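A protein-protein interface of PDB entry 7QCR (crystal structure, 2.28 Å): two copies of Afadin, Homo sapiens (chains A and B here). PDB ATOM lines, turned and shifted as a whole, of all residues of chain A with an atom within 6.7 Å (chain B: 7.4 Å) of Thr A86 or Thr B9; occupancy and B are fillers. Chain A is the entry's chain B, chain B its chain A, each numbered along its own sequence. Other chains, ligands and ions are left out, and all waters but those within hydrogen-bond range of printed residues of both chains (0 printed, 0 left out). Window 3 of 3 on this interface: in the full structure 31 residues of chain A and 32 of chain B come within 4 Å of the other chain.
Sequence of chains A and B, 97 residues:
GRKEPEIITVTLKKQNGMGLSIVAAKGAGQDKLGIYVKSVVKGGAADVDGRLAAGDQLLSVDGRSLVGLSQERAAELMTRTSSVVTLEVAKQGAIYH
O of Thr B9 lies within hydrogen-bond range of NH1 of Arg A51, 3.3 Å away.
O of Ile B8 sits at hydrogen-bond distance from N of Val A89 (2.8 Å).
OG1 of Thr A86 lies within hydrogen-bond range of OG1 of Thr B11 (3.0 Å).
O of Leu B12 sits at hydrogen-bond distance from N of Val A85, at 2.9 Å.
The backbone carbonyl oxygen (O) of Leu A87 is in hydrogen-bond range of the backbone NH (N) of Val B10 (2.9 Å).
The side-chain hydroxyl (OG) of Ser A60 sits at hydrogen-bond distance from the side-chain carboxylate (OE2) of Glu A88.
The side-chain carboxylate of Asp A62 is in hydrogen-bond range of the backbone NH of Thr A86.
Arg A51 touches Thr B11.
Val A84 touches Thr B11 (CG1 to CG2, 3.5 Å).
Leu B12 touches Val A84.
Val A85 touches Thr B11 (O to CA, 3.5 Å).
Thr A86 touches Thr B9 (CG2 to CG2, 3.9 Å).
Val B10 touches Thr A86.
O of Leu A87 touches CA of Thr B9 (3.6 Å).
Ile B8 touches Glu A88 (O to C, 3.7 Å).
OG1 of Thr B9 touches OE1 of Glu A88, at 3.6 Å.
O of Val A89 touches CA of Ile B7 (3.3 Å).
Thr B9 touches four residues of chain A.
Of the printed residues of chain B, Glu A88 touches Ile B8 (3.7 Å) and Thr B9 (3.6 Å).
Of the printed residues of chain B, Leu A87 touches Thr B9 (3.6 Å) and Val B10 (2.9 Å).
Printed residues of chain A within 4 Å of Ile B7: Val A89.
Val A61 touches none of the printed residues of chain B.
The nearest residue of chain B that does not touch Thr A86 is Leu B12 (5.1 Å).
The nearest residue of chain A that does not touch Thr B9 is Val A89 (4.9 Å).
Of the 6 printed residues of chain B, 6 touch a printed residue of chain A.
Hydrophobic or aromatic side chains of chain B that line the printed part of chain A: Ile B7 and Val B10.
Of the 12 printed residues of chain A, 7 touch a printed residue of chain B.
Printed residues of chain A that touch a printed residue of chain B: Arg A51, Val A84, Val A85, Thr A86, Leu A87, Glu A88 and Val A89.
Among the printed residues, no Asp or Glu carboxylate lies within 4 Å of a Lys or Arg side-chain nitrogen of the other chain.
No position is printed for both chains.
Of the 16 pairs that touch across the chains among the printed residues, none has its exchanged pair printed and touching as well.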
ATOM      1  N   ARG A  51       9.471  12.840  29.614  1.00  0.00           N
ATOM      2  CA  ARG A  51      10.138  11.974  30.585  1.00  0.00           C
ATOM      3  C   ARG A  51      11.658  11.921  30.427  1.00  0.00           C
ATOM      4  O   ARG A  51      12.347  11.859  31.443  1.00  0.00           O
ATOM      5  CB  ARG A  51       9.545  10.564  30.580  1.00  0.00           C
ATOM      6  CG  ARG A  51       8.095  10.500  31.013  1.00  0.00           C
ATOM      7  CD  ARG A  51       7.587   9.072  30.890  1.00  0.00           C
ATOM      8  NE  ARG A  51       7.216   8.738  29.512  1.00  0.00           N
ATOM      9  CZ  ARG A  51       6.812   7.534  29.112  1.00  0.00           C
ATOM     10  NH1 ARG A  51       6.777   6.520  29.966  1.00  0.00           N
ATOM     11  NH2 ARG A  51       6.446   7.336  27.855  1.00  0.00           N
ATOM     12  N   SER A  60      18.400   0.076  26.594  1.00  0.00           N
ATOM     13  CA  SER A  60      18.012  -0.813  25.504  1.00  0.00           C
ATOM     14  C   SER A  60      17.002  -0.184  24.537  1.00  0.00           C
ATOM     15  O   SER A  60      16.366   0.816  24.863  1.00  0.00           O
ATOM     16  CB  SER A  60      17.464  -2.130  26.052  1.00  0.00           C
ATOM     17  OG  SER A  60      16.152  -1.978  26.564  1.00  0.00           O
ATOM     18  N   VAL A  61      16.882  -0.785  23.337  1.00  0.00           N
ATOM     19  CA  VAL A  61      15.931  -0.460  22.272  1.00  0.00           C
ATOM     20  C   VAL A  61      15.220  -1.743  21.945  1.00  0.00           C
ATOM     21  O   VAL A  61      15.879  -2.696  21.551  1.00  0.00           O
ATOM     22  CB  VAL A  61      16.529   0.102  20.947  1.00  0.00           C
ATOM     23  CG1 VAL A  61      16.183   1.562  20.772  1.00  0.00           C
ATOM     24  CG2 VAL A  61      18.027  -0.176  20.780  1.00  0.00           C
ATOM     25  N   ASP A  62      13.896  -1.788  22.093  1.00  0.00           N
ATOM     26  CA  ASP A  62      13.091  -2.972  21.775  1.00  0.00           C
ATOM     27  C   ASP A  62      13.677  -4.318  22.276  1.00  0.00           C
ATOM     28  O   ASP A  62      13.723  -5.289  21.521  1.00  0.00           O
ATOM     29  CB  ASP A  62      12.803  -3.023  20.271  1.00  0.00           C
ATOM     30  CG  ASP A  62      12.058  -1.806  19.761  1.00  0.00           C
ATOM     31  OD1 ASP A  62      11.310  -1.199  20.548  1.00  0.00           O
ATOM     32  OD2 ASP A  62      12.211  -1.475  18.566  1.00  0.00           O
ATOM     33  N   GLY A  63      14.124  -4.342  23.534  1.00  0.00           N
ATOM     34  CA  GLY A  63      14.677  -5.541  24.150  1.00  0.00           C
ATOM     35  C   GLY A  63      16.136  -5.835  23.852  1.00  0.00           C
ATOM     36  O   GLY A  63      16.702  -6.767  24.425  1.00  0.00           O
ATOM     37  N   THR A  81      14.386   0.574  13.467  1.00  0.00           N
ATOM     38  CA  THR A  81      13.119   0.138  14.073  1.00  0.00           C
ATOM     39  C   THR A  81      11.872   0.773  13.376  1.00  0.00           C
ATOM     40  O   THR A  81      12.023   1.567  12.443  1.00  0.00           O
ATOM     41  CB  THR A  81      13.182   0.382  15.611  1.00  0.00           C
ATOM     42  OG1 THR A  81      11.924   0.054  16.224  1.00  0.00           O
ATOM     43  CG2 THR A  81      13.587   1.795  15.966  1.00  0.00           C
ATOM     44  N   VAL A  84       7.016   3.125  16.244  1.00  0.00           N
ATOM     45  CA  VAL A  84       7.017   3.138  17.699  1.00  0.00           C
ATOM     46  C   VAL A  84       8.181   2.308  18.272  1.00  0.00           C
ATOM     47  O   VAL A  84       8.340   1.136  17.929  1.00  0.00           O
ATOM     48  CB  VAL A  84       5.650   2.717  18.265  1.00  0.00           C
ATOM     49  CG1 VAL A  84       5.641   2.812  19.780  1.00  0.00           C
ATOM     50  CG2 VAL A  84       4.533   3.569  17.666  1.00  0.00           C
ATOM     51  N   VAL A  85       9.005   2.937  19.127  1.00  0.00           N
ATOM     52  CA  VAL A  85      10.193   2.319  19.726  1.00  0.00           C
ATOM     53  C   VAL A  85      10.119   2.326  21.256  1.00  0.00           C
ATOM     54  O   VAL A  85       9.667   3.303  21.847  1.00  0.00           O
ATOM     55  CB  VAL A  85      11.497   2.981  19.185  1.00  0.00           C
ATOM     56  CG1 VAL A  85      11.410   4.501  19.211  1.00  0.00           C
ATOM     57  CG2 VAL A  85      12.735   2.494  19.928  1.00  0.00           C
ATOM     58  N   THR A  86      10.528   1.226  21.898  1.00  0.00           N
ATOM     59  CA  THR A  86      10.502   1.115  23.352  1.00  0.00           C
ATOM     60  C   THR A  86      11.903   1.198  23.946  1.00  0.00           C
ATOM     61  O   THR A  86      12.749   0.358  23.659  1.00  0.00           O
ATOM     62  CB  THR A  86       9.776  -0.168  23.772  1.00  0.00           C
ATOM     63  OG1 THR A  86       8.419  -0.073  23.353  1.00  0.00           O
ATOM     64  CG2 THR A  86       9.822  -0.403  25.271  1.00  0.00           C
ATOM     65  N   LEU A  87      12.139   2.198  24.789  1.00  0.00           N
ATOM     66  CA  LEU A  87      13.432   2.377  25.432  1.00  0.00           C
ATOM     67  C   LEU A  87      13.358   2.058  26.927  1.00  0.00           C
ATOM     68  O   LEU A  87      12.410   2.457  27.594  1.00  0.00           O
ATOM     69  CB  LEU A  87      13.897   3.838  25.280  1.00  0.00           C
ATOM     70  CG  LEU A  87      14.050   4.409  23.852  1.00  0.00           C
ATOM     71  CD1 LEU A  87      13.984   5.920  23.863  1.00  0.00           C
ATOM     72  CD2 LEU A  87      15.364   3.993  23.239  1.00  0.00           C
ATOM     73  N   GLU A  88      14.380   1.374  27.460  1.00  0.00           N
ATOM     74  CA  GLU A  88      14.538   1.147  28.908  1.00  0.00           C
ATOM     75  C   GLU A  88      15.522   2.254  29.314  1.00  0.00           C
ATOM     76  O   GLU A  88      16.556   2.411  28.659  1.00  0.00           O
ATOM     77  CB  GLU A  88      15.157  -0.226  29.187  1.00  0.00           C
ATOM     78  CG  GLU A  88      14.329  -1.097  30.105  1.00  0.00           C
ATOM     79  CD  GLU A  88      13.927  -2.440  29.516  1.00  0.00           C
ATOM     80  OE1 GLU A  88      12.722  -2.775  29.597  1.00  0.00           O
ATOM     81  OE2 GLU A  88      14.804  -3.152  28.968  1.00  0.00           O
ATOM     82  N   VAL A  89      15.179   3.070  30.311  1.00  0.00           N
ATOM     83  CA  VAL A  89      15.998   4.233  30.660  1.00  0.00           C
ATOM     84  C   VAL A  89      16.441   4.236  32.121  1.00  0.00           C
ATOM     85  O   VAL A  89      15.636   3.978  33.001  1.00  0.00           O
ATOM     86  CB  VAL A  89      15.209   5.540  30.305  1.00  0.00           C
ATOM     87  CG1 VAL A  89      15.965   6.802  30.710  1.00  0.00           C
ATOM     88  CG2 VAL A  89      14.833   5.582  28.821  1.00  0.00           C
ATOM     89  N   ILE B   7      14.876   3.255  37.204  1.00  0.00           N
ATOM     90  CA  ILE B   7      14.789   2.668  35.863  1.00  0.00           C
ATOM     91  C   ILE B   7      13.349   2.647  35.369  1.00  0.00           C
ATOM     92  O   ILE B   7      12.511   1.933  35.923  1.00  0.00           O
ATOM     93  CB  ILE B   7      15.484   1.291  35.755  1.00  0.00           C
ATOM     94  CG1 ILE B   7      16.992   1.441  36.035  1.00  0.00           C
ATOM     95  CG2 ILE B   7      15.228   0.666  34.378  1.00  0.00           C
ATOM     96  CD1 ILE B   7      17.774   0.173  36.004  1.00  0.00           C
ATOM     97  N   ILE B   8      13.063   3.444  34.335  1.00  0.00           N
ATOM     98  CA  ILE B   8      11.727   3.573  33.767  1.00  0.00           C
ATOM     99  C   ILE B   8      11.672   3.035  32.326  1.00  0.00           C
ATOM    100  O   ILE B   8      12.710   2.842  31.695  1.00  0.00           O
ATOM    101  CB  ILE B   8      11.308   5.064  33.846  1.00  0.00           C
ATOM    102  CG1 ILE B   8       9.780   5.240  33.864  1.00  0.00           C
ATOM    103  CG2 ILE B   8      11.971   5.898  32.754  1.00  0.00           C
ATOM    104  CD1 ILE B   8       9.293   6.645  34.360  1.00  0.00           C
ATOM    105  N   THR B   9      10.465   2.768  31.805  1.00  0.00           N
ATOM    106  CA  THR B   9      10.298   2.276  30.444  1.00  0.00           C
ATOM    107  C   THR B   9       9.529   3.326  29.660  1.00  0.00           C
ATOM    108  O   THR B   9       8.391   3.644  29.996  1.00  0.00           O
ATOM    109  CB  THR B   9       9.654   0.885  30.430  1.00  0.00           C
ATOM    110  OG1 THR B   9      10.623  -0.075  30.864  1.00  0.00           O
ATOM    111  CG2 THR B   9       9.165   0.487  29.054  1.00  0.00           C
ATOM    112  N   VAL B  10      10.177   3.915  28.658  1.00  0.00           N
ATOM    113  CA  VAL B  10       9.590   4.980  27.859  1.00  0.00           C
ATOM    114  C   VAL B  10       9.352   4.549  26.426  1.00  0.00           C
ATOM    115  O   VAL B  10      10.298   4.237  25.711  1.00  0.00           O
ATOM    116  CB  VAL B  10      10.460   6.250  27.918  1.00  0.00           C
ATOM    117  CG1 VAL B  10       9.863   7.362  27.068  1.00  0.00           C
ATOM    118  CG2 VAL B  10      10.656   6.709  29.358  1.00  0.00           C
ATOM    119  N   THR B  11       8.094   4.542  26.007  1.00  0.00           N
ATOM    120  CA  THR B  11       7.740   4.177  24.645  1.00  0.00           C
ATOM    121  C   THR B  11       7.440   5.446  23.854  1.00  0.00           C
ATOM    122  O   THR B  11       6.655   6.281  24.300  1.00  0.00           O
ATOM    123  CB  THR B  11       6.610   3.148  24.664  1.00  0.00           C
ATOM    124  OG1 THR B  11       7.110   1.935  25.228  1.00  0.00           O
ATOM    125  CG2 THR B  11       6.064   2.871  23.294  1.00  0.00           C
ATOM    126  N   LEU B  12       8.122   5.632  22.719  1.00  0.00           N
ATOM    127  CA  LEU B  12       7.934   6.830  21.911  1.00  0.00           C
ATOM    128  C   LEU B  12       7.510   6.484  20.514  1.00  0.00           C
ATOM    129  O   LEU B  12       8.029   5.538  19.917  1.00  0.00           O
ATOM    130  CB  LEU B  12       9.239   7.649  21.812  1.00  0.00           C
ATOM    131  CG  LEU B  12       9.886   8.104  23.105  1.00  0.00           C
ATOM    132  CD1 LEU B  12      11.272   8.681  22.840  1.00  0.00           C
ATOM    133  CD2 LEU B  12       9.018   9.105  23.815  1.00  0.00           C
